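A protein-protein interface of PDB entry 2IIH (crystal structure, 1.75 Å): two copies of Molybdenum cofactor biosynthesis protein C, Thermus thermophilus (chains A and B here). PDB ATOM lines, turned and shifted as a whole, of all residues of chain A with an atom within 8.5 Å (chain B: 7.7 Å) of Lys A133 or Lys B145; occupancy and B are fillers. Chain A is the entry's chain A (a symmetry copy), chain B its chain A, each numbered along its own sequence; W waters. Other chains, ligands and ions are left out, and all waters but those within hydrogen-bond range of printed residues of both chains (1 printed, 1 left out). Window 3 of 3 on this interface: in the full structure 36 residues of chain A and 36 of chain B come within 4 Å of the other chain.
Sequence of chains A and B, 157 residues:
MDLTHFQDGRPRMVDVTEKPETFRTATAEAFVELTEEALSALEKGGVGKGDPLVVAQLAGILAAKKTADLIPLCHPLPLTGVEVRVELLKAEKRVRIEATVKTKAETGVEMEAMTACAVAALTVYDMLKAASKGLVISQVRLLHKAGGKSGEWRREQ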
ATOM      1  N   THR A  35     -35.255  -9.905  22.359  1.00  0.00           N
ATOM      2  CA  THR A  35     -35.752  -9.543  21.039  1.00  0.00           C
ATOM      3  C   THR A  35     -36.540 -10.788  20.646  1.00  0.00           C
ATOM      4  O   THR A  35     -36.456 -11.800  21.338  1.00  0.00           O
ATOM      5  CB  THR A  35     -34.604  -9.336  20.029  1.00  0.00           C
ATOM      6  OG1 THR A  35     -33.736 -10.475  20.052  1.00  0.00           O
ATOM      7  CG2 THR A  35     -33.809  -8.084  20.367  1.00  0.00           C
ATOM      8  N   GLU A  37     -35.992 -12.726  18.211  1.00  0.00           N
ATOM      9  CA  GLU A  37     -35.009 -13.732  17.825  1.00  0.00           C
ATOM     10  C   GLU A  37     -34.478 -14.464  19.056  1.00  0.00           C
ATOM     11  O   GLU A  37     -34.341 -15.689  19.049  1.00  0.00           O
ATOM     12  CB  GLU A  37     -33.844 -13.076  17.075  1.00  0.00           C
ATOM     13  CG  GLU A  37     -34.262 -12.122  15.965  1.00  0.00           C
ATOM     14  CD  GLU A  37     -34.452 -10.697  16.453  1.00  0.00           C
ATOM     15  OE1 GLU A  37     -33.441 -10.039  16.775  1.00  0.00           O
ATOM     16  OE2 GLU A  37     -35.611 -10.235  16.521  1.00  0.00           O
ATOM     17  N   ALA A  38     -34.181 -13.712  20.111  1.00  0.00           N
ATOM     18  CA  ALA A  38     -33.660 -14.294  21.346  1.00  0.00           C
ATOM     19  C   ALA A  38     -34.713 -15.139  22.059  1.00  0.00           C
ATOM     20  O   ALA A  38     -34.410 -16.207  22.592  1.00  0.00           O
ATOM     21  CB  ALA A  38     -33.160 -13.184  22.272  1.00  0.00           C
ATOM     22  N   TYR A 125     -26.837 -13.423  28.627  1.00  0.00           N
ATOM     23  CA  TYR A 125     -26.373 -12.645  27.482  1.00  0.00           C
ATOM     24  C   TYR A 125     -25.333 -13.433  26.690  1.00  0.00           C
ATOM     25  O   TYR A 125     -25.396 -13.511  25.461  1.00  0.00           O
ATOM     26  CB  TYR A 125     -25.741 -11.322  27.946  1.00  0.00           C
ATOM     27  CG  TYR A 125     -25.154 -10.507  26.815  1.00  0.00           C
ATOM     28  CD1 TYR A 125     -25.972  -9.748  25.979  1.00  0.00           C
ATOM     29  CD2 TYR A 125     -23.786 -10.542  26.539  1.00  0.00           C
ATOM     30  CE1 TYR A 125     -25.441  -9.043  24.894  1.00  0.00           C
ATOM     31  CE2 TYR A 125     -23.246  -9.843  25.457  1.00  0.00           C
ATOM     32  CZ  TYR A 125     -24.081  -9.100  24.638  1.00  0.00           C
ATOM     33  OH  TYR A 125     -23.559  -8.429  23.554  1.00  0.00           O
ATOM     34  N   LEU A 128     -26.832 -16.001  24.319  1.00  0.00           N
ATOM     35  CA  LEU A 128     -27.838 -15.547  23.362  1.00  0.00           C
ATOM     36  C   LEU A 128     -27.280 -14.453  22.461  1.00  0.00           C
ATOM     37  O   LEU A 128     -27.922 -14.058  21.488  1.00  0.00           O
ATOM     38  CB  LEU A 128     -29.078 -15.016  24.082  1.00  0.00           C
ATOM     39  CG  LEU A 128     -29.971 -16.008  24.825  1.00  0.00           C
ATOM     40  CD1 LEU A 128     -31.081 -15.247  25.530  1.00  0.00           C
ATOM     41  CD2 LEU A 128     -30.548 -17.021  23.848  1.00  0.00           C
ATOM     42  N   LYS A 129     -26.081 -13.969  22.772  1.00  0.00           N
ATOM     43  CA  LYS A 129     -25.476 -12.901  21.981  1.00  0.00           C
ATOM     44  C   LYS A 129     -25.132 -13.315  20.551  1.00  0.00           C
ATOM     45  O   LYS A 129     -24.924 -12.463  19.686  1.00  0.00           O
ATOM     46  CB  LYS A 129     -24.224 -12.357  22.679  1.00  0.00           C
ATOM     47  CG  LYS A 129     -23.008 -13.264  22.634  1.00  0.00           C
ATOM     48  CD  LYS A 129     -21.842 -12.613  23.367  1.00  0.00           C
ATOM     49  CE  LYS A 129     -20.543 -13.364  23.144  1.00  0.00           C
ATOM     50  NZ  LYS A 129     -20.659 -14.794  23.515  1.00  0.00           N
ATOM     51  N   ALA A 130     -25.072 -14.618  20.301  1.00  0.00           N
ATOM     52  CA  ALA A 130     -24.760 -15.112  18.966  1.00  0.00           C
ATOM     53  C   ALA A 130     -25.883 -14.725  18.008  1.00  0.00           C
ATOM     54  O   ALA A 130     -25.644 -14.444  16.835  1.00  0.00           O
ATOM     55  CB  ALA A 130     -24.590 -16.624  18.989  1.00  0.00           C
ATOM     56  N   ALA A 131     -27.108 -14.709  18.520  1.00  0.00           N
ATOM     57  CA  ALA A 131     -28.270 -14.353  17.715  1.00  0.00           C
ATOM     58  C   ALA A 131     -28.654 -12.887  17.899  1.00  0.00           C
ATOM     59  O   ALA A 131     -29.229 -12.275  16.998  1.00  0.00           O
ATOM     60  CB  ALA A 131     -29.449 -15.250  18.083  1.00  0.00           C
ATOM     61  N   SER A 132     -28.333 -12.321  19.060  1.00  0.00           N
ATOM     62  CA  SER A 132     -28.665 -10.927  19.341  1.00  0.00           C
ATOM     63  C   SER A 132     -27.628 -10.235  20.223  1.00  0.00           C
ATOM     64  O   SER A 132     -27.691 -10.307  21.450  1.00  0.00           O
ATOM     65  CB  SER A 132     -30.036 -10.850  20.009  1.00  0.00           C
ATOM     66  OG  SER A 132     -31.013 -11.519  19.231  1.00  0.00           O
ATOM     67  N   LYS A 133     -26.681  -9.554  19.589  1.00  0.00           N
ATOM     68  CA  LYS A 133     -25.636  -8.855  20.322  1.00  0.00           C
ATOM     69  C   LYS A 133     -26.136  -7.605  21.037  1.00  0.00           C
ATOM     70  O   LYS A 133     -25.466  -7.092  21.934  1.00  0.00           O
ATOM     71  CB  LYS A 133     -24.489  -8.500  19.371  1.00  0.00           C
ATOM     72  CG  LYS A 133     -23.741  -9.729  18.889  1.00  0.00           C
ATOM     73  CD  LYS A 133     -22.749  -9.421  17.792  1.00  0.00           C
ATOM     74  CE  LYS A 133     -22.079 -10.704  17.325  1.00  0.00           C
ATOM     75  NZ  LYS A 133     -23.079 -11.747  16.957  1.00  0.00           N
ATOM     76  N   GLY A 134     -27.322  -7.135  20.650  1.00  0.00           N
ATOM     77  CA  GLY A 134     -27.887  -5.939  21.256  1.00  0.00           C
ATOM     78  C   GLY A 134     -28.714  -6.133  22.517  1.00  0.00           C
ATOM     79  O   GLY A 134     -29.240  -5.160  23.059  1.00  0.00           O
ATOM     80  N   LEU A 135     -28.843  -7.372  22.988  1.00  0.00           N
ATOM     81  CA  LEU A 135     -29.618  -7.648  24.198  1.00  0.00           C
ATOM     82  C   LEU A 135     -29.125  -6.805  25.366  1.00  0.00           C
ATOM     83  O   LEU A 135     -27.916  -6.680  25.587  1.00  0.00           O
ATOM     84  CB  LEU A 135     -29.532  -9.132  24.568  1.00  0.00           C
ATOM     85  CG  LEU A 135     -30.201 -10.109  23.596  1.00  0.00           C
ATOM     86  CD1 LEU A 135     -30.040 -11.530  24.098  1.00  0.00           C
ATOM     87  CD2 LEU A 135     -31.674  -9.764  23.454  1.00  0.00           C
ATOM     88  N   VAL A 136     -30.068  -6.247  26.119  1.00  0.00           N
ATOM     89  CA  VAL A 136     -29.748  -5.392  27.250  1.00  0.00           C
ATOM     90  C   VAL A 136     -30.071  -5.989  28.612  1.00  0.00           C
ATOM     91  O   VAL A 136     -31.114  -6.628  28.804  1.00  0.00           O
ATOM     92  CB  VAL A 136     -30.498  -4.039  27.140  1.00  0.00           C
ATOM     93  CG1 VAL A 136     -30.193  -3.167  28.349  1.00  0.00           C
ATOM     94  CG2 VAL A 136     -30.097  -3.328  25.863  1.00  0.00           C
ATOM     95  N   ARG B  24      -9.515  -8.694  17.918  1.00  0.00           N
ATOM     96  CA  ARG B  24     -10.883  -8.487  18.374  1.00  0.00           C
ATOM     97  C   ARG B  24     -10.975  -7.284  19.310  1.00  0.00           C
ATOM     98  O   ARG B  24     -10.020  -6.946  20.013  1.00  0.00           O
ATOM     99  CB  ARG B  24     -11.392  -9.724  19.122  1.00  0.00           C
ATOM    100  CG  ARG B  24     -11.199 -11.065  18.415  1.00  0.00           C
ATOM    101  CD  ARG B  24     -11.832 -11.079  17.041  1.00  0.00           C
ATOM    102  NE  ARG B  24     -11.826 -12.413  16.443  1.00  0.00           N
ATOM    103  CZ  ARG B  24     -12.834 -13.277  16.515  1.00  0.00           C
ATOM    104  NH1 ARG B  24     -13.948 -12.957  17.164  1.00  0.00           N
ATOM    105  NH2 ARG B  24     -12.739 -14.456  15.917  1.00  0.00           N
ATOM    106  N   THR B  25     -12.136  -6.642  19.314  1.00  0.00           N
ATOM    107  CA  THR B  25     -12.376  -5.506  20.185  1.00  0.00           C
ATOM    108  C   THR B  25     -13.854  -5.484  20.549  1.00  0.00           C
ATOM    109  O   THR B  25     -14.697  -5.954  19.786  1.00  0.00           O
ATOM    110  CB  THR B  25     -12.004  -4.169  19.508  1.00  0.00           C
ATOM    111  OG1 THR B  25     -12.189  -3.098  20.440  1.00  0.00           O
ATOM    112  CG2 THR B  25     -12.884  -3.919  18.300  1.00  0.00           C
ATOM    113  N   ALA B  26     -14.157  -4.957  21.730  1.00  0.00           N
ATOM    114  CA  ALA B  26     -15.535  -4.859  22.188  1.00  0.00           C
ATOM    115  C   ALA B  26     -15.660  -3.692  23.154  1.00  0.00           C
ATOM    116  O   ALA B  26     -14.758  -3.439  23.957  1.00  0.00           O
ATOM    117  CB  ALA B  26     -15.969  -6.159  22.867  1.00  0.00           C
ATOM    118  N   THR B  27     -16.780  -2.983  23.064  1.00  0.00           N
ATOM    119  CA  THR B  27     -17.043  -1.836  23.924  1.00  0.00           C
ATOM    120  C   THR B  27     -18.458  -1.942  24.483  1.00  0.00           C
ATOM    121  O   THR B  27     -19.413  -2.181  23.740  1.00  0.00           O
ATOM    122  CB  THR B  27     -16.926  -0.503  23.138  1.00  0.00           C
ATOM    123  OG1 THR B  27     -15.621  -0.401  22.555  1.00  0.00           O
ATOM    124  CG2 THR B  27     -17.155   0.683  24.057  1.00  0.00           C
ATOM    125  N   ALA B  28     -18.588  -1.776  25.794  1.00  0.00           N
ATOM    126  CA  ALA B  28     -19.891  -1.841  26.440  1.00  0.00           C
ATOM    127  C   ALA B  28     -20.029  -0.692  27.424  1.00  0.00           C
ATOM    128  O   ALA B  28     -19.071   0.037  27.681  1.00  0.00           O
ATOM    129  CB  ALA B  28     -20.053  -3.178  27.173  1.00  0.00           C
ATOM    130  N   VAL B 101     -12.315  -3.549  25.557  1.00  0.00           N
ATOM    131  CA  VAL B 101     -11.344  -4.624  25.713  1.00  0.00           C
ATOM    132  C   VAL B 101     -10.844  -5.066  24.340  1.00  0.00           C
ATOM    133  O   VAL B 101     -11.596  -5.050  23.366  1.00  0.00           O
ATOM    134  CB  VAL B 101     -11.984  -5.823  26.435  1.00  0.00           C
ATOM    135  CG1 VAL B 101     -10.973  -6.963  26.573  1.00  0.00           C
ATOM    136  CG2 VAL B 101     -12.484  -5.383  27.801  1.00  0.00           C
ATOM    137  N   GLY B 108     -14.581 -13.529  20.333  1.00  0.00           N
ATOM    138  CA  GLY B 108     -14.673 -12.132  20.723  1.00  0.00           C
ATOM    139  C   GLY B 108     -14.544 -11.826  22.205  1.00  0.00           C
ATOM    140  O   GLY B 108     -14.525 -12.726  23.046  1.00  0.00           O
ATOM    141  N   VAL B 109     -14.453 -10.541  22.528  1.00  0.00           N
ATOM    142  CA  VAL B 109     -14.330 -10.115  23.915  1.00  0.00           C
ATOM    143  C   VAL B 109     -15.526  -9.306  24.395  1.00  0.00           C
ATOM    144  O   VAL B 109     -15.400  -8.432  25.258  1.00  0.00           O
ATOM    145  CB  VAL B 109     -13.027  -9.313  24.140  1.00  0.00           C
ATOM    146  CG1 VAL B 109     -11.843 -10.255  24.086  1.00  0.00           C
ATOM    147  CG2 VAL B 109     -12.876  -8.213  23.080  1.00  0.00           C
ATOM    148  N   GLU B 110     -16.695  -9.613  23.841  1.00  0.00           N
ATOM    149  CA  GLU B 110     -17.913  -8.930  24.241  1.00  0.00           C
ATOM    150  C   GLU B 110     -18.159  -9.182  25.723  1.00  0.00           C
ATOM    151  O   GLU B 110     -18.508  -8.267  26.463  1.00  0.00           O
ATOM    152  CB  GLU B 110     -19.113  -9.429  23.434  1.00  0.00           C
ATOM    153  CG  GLU B 110     -19.018  -9.124  21.949  1.00  0.00           C
ATOM    154  CD  GLU B 110     -18.457 -10.274  21.143  1.00  0.00           C
ATOM    155  OE1 GLU B 110     -17.667 -11.066  21.697  1.00  0.00           O
ATOM    156  OE2 GLU B 110     -18.802 -10.375  19.945  1.00  0.00           O
ATOM    157  N   MET B 114     -18.581  -6.384  28.698  1.00  0.00           N
ATOM    158  CA  MET B 114     -19.827  -6.390  29.458  1.00  0.00           C
ATOM    159  C   MET B 114     -19.586  -6.638  30.948  1.00  0.00           C
ATOM    160  O   MET B 114     -20.167  -5.964  31.796  1.00  0.00           O
ATOM    161  CB  MET B 114     -20.772  -7.467  28.914  1.00  0.00           C
ATOM    162  CG  MET B 114     -21.361  -7.173  27.540  1.00  0.00           C
ATOM    163  SD  MET B 114     -22.636  -5.897  27.595  1.00  0.00           S
ATOM    164  CE  MET B 114     -24.077  -6.873  28.120  1.00  0.00           C
ATOM    165  N   ARG B 141     -25.072  -2.822  28.447  1.00  0.00           N
ATOM    166  CA  ARG B 141     -25.263  -3.191  27.049  1.00  0.00           C
ATOM    167  C   ARG B 141     -24.022  -3.002  26.197  1.00  0.00           C
ATOM    168  O   ARG B 141     -23.147  -2.191  26.517  1.00  0.00           O
ATOM    169  CB  ARG B 141     -26.400  -2.349  26.466  1.00  0.00           C
ATOM    170  CG  ARG B 141     -26.117  -0.857  26.536  1.00  0.00           C
ATOM    171  CD  ARG B 141     -27.335  -0.017  26.173  1.00  0.00           C
ATOM    172  NE  ARG B 141     -27.067   1.405  26.359  1.00  0.00           N
ATOM    173  CZ  ARG B 141     -27.913   2.377  26.035  1.00  0.00           C
ATOM    174  NH1 ARG B 141     -29.092   2.087  25.503  1.00  0.00           N
ATOM    175  NH2 ARG B 141     -27.578   3.643  26.243  1.00  0.00           N
ATOM    176  N   LEU B 142     -23.969  -3.746  25.099  1.00  0.00           N
ATOM    177  CA  LEU B 142     -22.850  -3.681  24.170  1.00  0.00           C
ATOM    178  C   LEU B 142     -23.052  -2.496  23.234  1.00  0.00           C
ATOM    179  O   LEU B 142     -24.168  -2.245  22.768  1.00  0.00           O
ATOM    180  CB  LEU B 142     -22.761  -4.976  23.353  1.00  0.00           C
ATOM    181  CG  LEU B 142     -21.450  -5.178  22.577  1.00  0.00           C
ATOM    182  CD1 LEU B 142     -20.314  -5.386  23.573  1.00  0.00           C
ATOM    183  CD2 LEU B 142     -21.558  -6.379  21.645  1.00  0.00           C
ATOM    184  N   LEU B 143     -21.973  -1.771  22.964  1.00  0.00           N
ATOM    185  CA  LEU B 143     -22.033  -0.611  22.081  1.00  0.00           C
ATOM    186  C   LEU B 143     -21.357  -0.882  20.745  1.00  0.00           C
ATOM    187  O   LEU B 143     -21.773  -0.357  19.706  1.00  0.00           O
ATOM    188  CB  LEU B 143     -21.358   0.594  22.741  1.00  0.00           C
ATOM    189  CG  LEU B 143     -21.944   1.104  24.058  1.00  0.00           C
ATOM    190  CD1 LEU B 143     -21.174   2.343  24.495  1.00  0.00           C
ATOM    191  CD2 LEU B 143     -23.430   1.420  23.890  1.00  0.00           C
ATOM    192  N   HIS B 144     -20.316  -1.705  20.764  1.00  0.00           N
ATOM    193  CA  HIS B 144     -19.583  -1.993  19.541  1.00  0.00           C
ATOM    194  C   HIS B 144     -18.668  -3.200  19.681  1.00  0.00           C
ATOM    195  O   HIS B 144     -18.327  -3.618  20.786  1.00  0.00           O
ATOM    196  CB  HIS B 144     -18.774  -0.745  19.149  1.00  0.00           C
ATOM    197  CG  HIS B 144     -17.831  -0.956  18.003  1.00  0.00           C
ATOM    198  ND1 HIS B 144     -16.584  -1.524  18.158  1.00  0.00           N
ATOM    199  CD2 HIS B 144     -17.957  -0.679  16.684  1.00  0.00           C
ATOM    200  CE1 HIS B 144     -15.982  -1.586  16.984  1.00  0.00           C
ATOM    201  NE2 HIS B 144     -16.795  -1.081  16.073  1.00  0.00           N
ATOM    202  N   LYS B 145     -18.297  -3.770  18.543  1.00  0.00           N
ATOM    203  CA  LYS B 145     -17.394  -4.904  18.516  1.00  0.00           C
ATOM    204  C   LYS B 145     -16.899  -5.062  17.086  1.00  0.00           C
ATOM    205  O   LYS B 145     -17.612  -4.739  16.132  1.00  0.00           O
ATOM    206  CB  LYS B 145     -18.101  -6.181  18.996  1.00  0.00           C
ATOM    207  CG  LYS B 145     -19.012  -6.872  17.982  1.00  0.00           C
ATOM    208  CD  LYS B 145     -18.220  -7.792  17.054  1.00  0.00           C
ATOM    209  CE  LYS B 145     -19.143  -8.626  16.185  1.00  0.00           C
ATOM    210  NZ  LYS B 145     -18.383  -9.564  15.311  1.00  0.00           N
ATOM    211  N   ALA B 146     -15.668  -5.535  16.952  1.00  0.00           N
ATOM    212  CA  ALA B 146     -15.057  -5.750  15.647  1.00  0.00           C
ATOM    213  C   ALA B 146     -14.316  -7.080  15.695  1.00  0.00           C
ATOM    214  O   ALA B 146     -13.978  -7.565  16.774  1.00  0.00           O
ATOM    215  CB  ALA B 146     -14.093  -4.615  15.322  1.00  0.00           C
ATOM    216  N   GLY B 147     -14.052  -7.656  14.526  1.00  0.00           N
ATOM    217  CA  GLY B 147     -13.377  -8.939  14.472  1.00  0.00           C
ATOM    218  C   GLY B 147     -14.426 -10.032  14.391  1.00  0.00           C
ATOM    219  O   GLY B 147     -15.568  -9.828  14.805  1.00  0.00           O
ATOM    220  N   GLY B 148     -14.049 -11.190  13.859  1.00  0.00           N
ATOM    221  CA  GLY B 148     -14.995 -12.284  13.725  1.00  0.00           C
ATOM    222  C   GLY B 148     -15.609 -12.292  12.335  1.00  0.00           C
ATOM    223  O   GLY B 148     -15.430 -11.346  11.570  1.00  0.00           O
ATOM    224  N   LYS B 149     -16.339 -13.353  12.005  1.00  0.00           N
ATOM    225  CA  LYS B 149     -16.967 -13.471  10.693  1.00  0.00           C
ATOM    226  C   LYS B 149     -18.073 -12.438  10.498  1.00  0.00           C
ATOM    227  O   LYS B 149     -18.187 -11.835   9.430  1.00  0.00           O
ATOM    228  CB  LYS B 149     -17.553 -14.870  10.512  1.00  0.00           C
ATOM    229  CG  LYS B 149     -18.091 -15.149   9.114  1.00  0.00           C
ATOM    230  CD  LYS B 149     -19.201 -16.182   9.175  1.00  0.00           C
ATOM    231  CE  LYS B 149     -19.492 -16.810   7.824  1.00  0.00           C
ATOM    232  NZ  LYS B 149     -20.620 -17.781   7.913  1.00  0.00           N
ATOM    233  N   SER B 150     -18.886 -12.238  11.532  1.00  0.00           N
ATOM    234  CA  SER B 150     -19.982 -11.278  11.462  1.00  0.00           C
ATOM    235  C   SER B 150     -19.453  -9.869  11.231  1.00  0.00           C
ATOM    236  O   SER B 150     -20.194  -8.971  10.831  1.00  0.00           O
ATOM    237  CB  SER B 150     -20.815 -11.323  12.747  1.00  0.00           C
ATOM    238  OG  SER B 150     -20.018 -11.070  13.891  1.00  0.00           O
ATOM    239  N   GLY B 151     -18.165  -9.681  11.488  1.00  0.00           N
ATOM    240  CA  GLY B 151     -17.555  -8.383  11.285  1.00  0.00           C
ATOM    241  C   GLY B 151     -17.932  -7.322  12.299  1.00  0.00           C
ATOM    242  O   GLY B 151     -18.320  -7.618  13.429  1.00  0.00           O
ATOM    243  N   GLU B 152     -17.818  -6.070  11.869  1.00  0.00           N
ATOM    244  CA  GLU B 152     -18.116  -4.916  12.703  1.00  0.00           C
ATOM    245  C   GLU B 152     -19.592  -4.834  13.080  1.00  0.00           C
ATOM    246  O   GLU B 152     -20.474  -5.079  12.255  1.00  0.00           O
ATOM    247  CB  GLU B 152     -17.703  -3.643  11.962  1.00  0.00           C
ATOM    248  CG  GLU B 152     -17.585  -2.396  12.823  1.00  0.00           C
ATOM    249  CD  GLU B 152     -16.162  -1.872  12.867  1.00  0.00           C
ATOM    250  OE1 GLU B 152     -15.374  -2.224  11.964  1.00  0.00           O
ATOM    251  OE2 GLU B 152     -15.830  -1.100  13.791  1.00  0.00           O
ATOM    252  N   TRP B 153     -19.855  -4.491  14.338  1.00  0.00           N
ATOM    253  CA  TRP B 153     -21.217  -4.345  14.835  1.00  0.00           C
ATOM    254  C   TRP B 153     -21.296  -3.041  15.615  1.00  0.00           C
ATOM    255  O   TRP B 153     -20.374  -2.693  16.352  1.00  0.00           O
ATOM    256  CB  TRP B 153     -21.598  -5.505  15.751  1.00  0.00           C
ATOM    257  CG  TRP B 153     -23.001  -5.398  16.272  1.00  0.00           C
ATOM    258  CD1 TRP B 153     -24.144  -5.809  15.646  1.00  0.00           C
ATOM    259  CD2 TRP B 153     -23.412  -4.823  17.518  1.00  0.00           C
ATOM    260  NE1 TRP B 153     -25.240  -5.532  16.428  1.00  0.00           N
ATOM    261  CE2 TRP B 153     -24.819  -4.930  17.587  1.00  0.00           C
ATOM    262  CE3 TRP B 153     -22.726  -4.236  18.592  1.00  0.00           C
ATOM    263  CZ2 TRP B 153     -25.557  -4.463  18.681  1.00  0.00           C
ATOM    264  CZ3 TRP B 153     -23.461  -3.773  19.682  1.00  0.00           C
ATOM    265  CH2 TRP B 153     -24.861  -3.895  19.719  1.00  0.00           C
ATOM    266  N   ARG B 154     -22.408  -2.330  15.464  1.00  0.00           N
ATOM    267  CA  ARG B 154     -22.590  -1.051  16.131  1.00  0.00           C
ATOM    268  C   ARG B 154     -24.028  -0.909  16.622  1.00  0.00           C
ATOM    269  O   ARG B 154     -24.967  -1.303  15.930  1.00  0.00           O
ATOM    270  CB  ARG B 154     -22.268   0.060  15.133  1.00  0.00           C
ATOM    271  CG  ARG B 154     -21.463   1.222  15.670  1.00  0.00           C
ATOM    272  CD  ARG B 154     -20.521   1.718  14.575  1.00  0.00           C
ATOM    273  NE  ARG B 154     -20.135   3.117  14.738  1.00  0.00           N
ATOM    274  CZ  ARG B 154     -19.098   3.680  14.128  1.00  0.00           C
ATOM    275  NH1 ARG B 154     -18.828   4.961  14.334  1.00  0.00           N
ATOM    276  NH2 ARG B 154     -18.325   2.959  13.327  1.00  0.00           N
ATOM    277  N   ARG B 155     -24.202  -0.358  17.818  1.00  0.00           N
ATOM    278  CA  ARG B 155     -25.541  -0.160  18.359  1.00  0.00           C
ATOM    279  C   ARG B 155     -26.124   1.126  17.782  1.00  0.00           C
ATOM    280  O   ARG B 155     -25.417   2.158  17.811  1.00  0.00           O
ATOM    281  CB  ARG B 155     -25.502  -0.063  19.888  1.00  0.00           C
ATOM    282  CG  ARG B 155     -26.829   0.353  20.522  1.00  0.00           C
ATOM    283  CD  ARG B 155     -26.724   0.390  22.038  1.00  0.00           C
ATOM    284  NE  ARG B 155     -26.418  -0.931  22.574  1.00  0.00           N
ATOM    285  CZ  ARG B 155     -27.299  -1.920  22.677  1.00  0.00           C
ATOM    286  NH1 ARG B 155     -26.926  -3.091  23.168  1.00  0.00           N
ATOM    287  NH2 ARG B 155     -28.561  -1.733  22.309  1.00  0.00           N
HETATM  288  O   HOH W   1     -31.384  -2.806  22.103  1.00  0.00           O
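The backbone carbonyl oxygen (O) of Gly A134 is in hydrogen-bond range of the guanidinium group (NH1) of Arg B155 (3.1 Å).
O of Leu B142 lies within hydrogen-bond range of NE of Arg B155 (2.6 Å).
The side-chain hydroxyl (OG) of Ser B150 is in hydrogen-bond range of the side-chain amino group (NZ) of Lys B145 (2.6 Å).
The backbone carbonyl oxygen (O) of Lys A129 lies close to the side-chain amino group (NZ) of Lys A133, at 3.4 Å.
The backbone carbonyl oxygen of Gly B151 lies within hydrogen-bond range of the side-chain amino group of Lys B145, at 2.7 Å.
The side-chain sulfur (SD) of Met B114 lies within hydrogen-bond range of the backbone NH (N) of Leu B142.
The side-chain hydroxyl of Tyr A125 sits at hydrogen-bond distance from the backbone carbonyl oxygen of Lys A133, 2.8 Å away.
Met B114 touches Tyr A125 (CG to CE2, 3.9 Å).
Tyr A125 touches Leu B142.
Lys A129 touches Glu B110 (CE to OE1, 3.96 Å).
Lys A133 touches Leu B142.
Lys B145 touches Lys A133 (CE to CE, 3.8 Å).
CH2 of Trp B153 touches O of Lys A133, at 3.9 Å.
Gly A134 touches Trp B153.
Val A136 touches Arg B141.
Of chain B, only Leu B142, Lys B145 and Trp B153 come within 4 Å of Lys A133.
Of chain A, only Lys A133 (3.8 Å) comes within 4 Å of Lys B145.
No residue of chain A comes within 4 Å of His B144.
Printed residues of chain A within 4 Å of Glu B110: Lys A129.
Printed residues of chain B within 4 Å of Lys A129: Glu B110.
Printed residues of chain B within 4 Å of Tyr A125: Met B114 (3.9 Å) and Leu B142 (3.4 Å).
Printed residues of chain A within 4 Å of Leu B142: Tyr A125 and Lys A133.
Of the printed residues of chain A, Met B114 touches Tyr A125 (3.9 Å).
Thr B27 touches none of the printed residues of chain A.
The nearest residue of chain B that does not touch Lys A133 is Ser B150 (4.02 Å).
The nearest printed residue of chain A that does not touch Glu B110 is Lys A133 (4.2 Å).
Of the 13 printed residues of chain A, 5 touch a printed residue of chain B.
Printed residues of chain A that touch a printed residue of chain B: Tyr A125, Lys A129, Lys A133, Gly A134 and Val A136.
Hydrophobic or aromatic side chains of chain A that line the printed part of chain B: Tyr A125 and Val A136.
Of the 25 printed residues of chain B, 7 touch a printed residue of chain A.
No position is printed for both chains.
Of the 9 pairs that touch across the chains among the printed residues, none has its exchanged pair printed and touching as well.
Water W1 bridges NH2 of Arg B155 (3.0 Å) and O of Gly A134 (3.3 Å).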
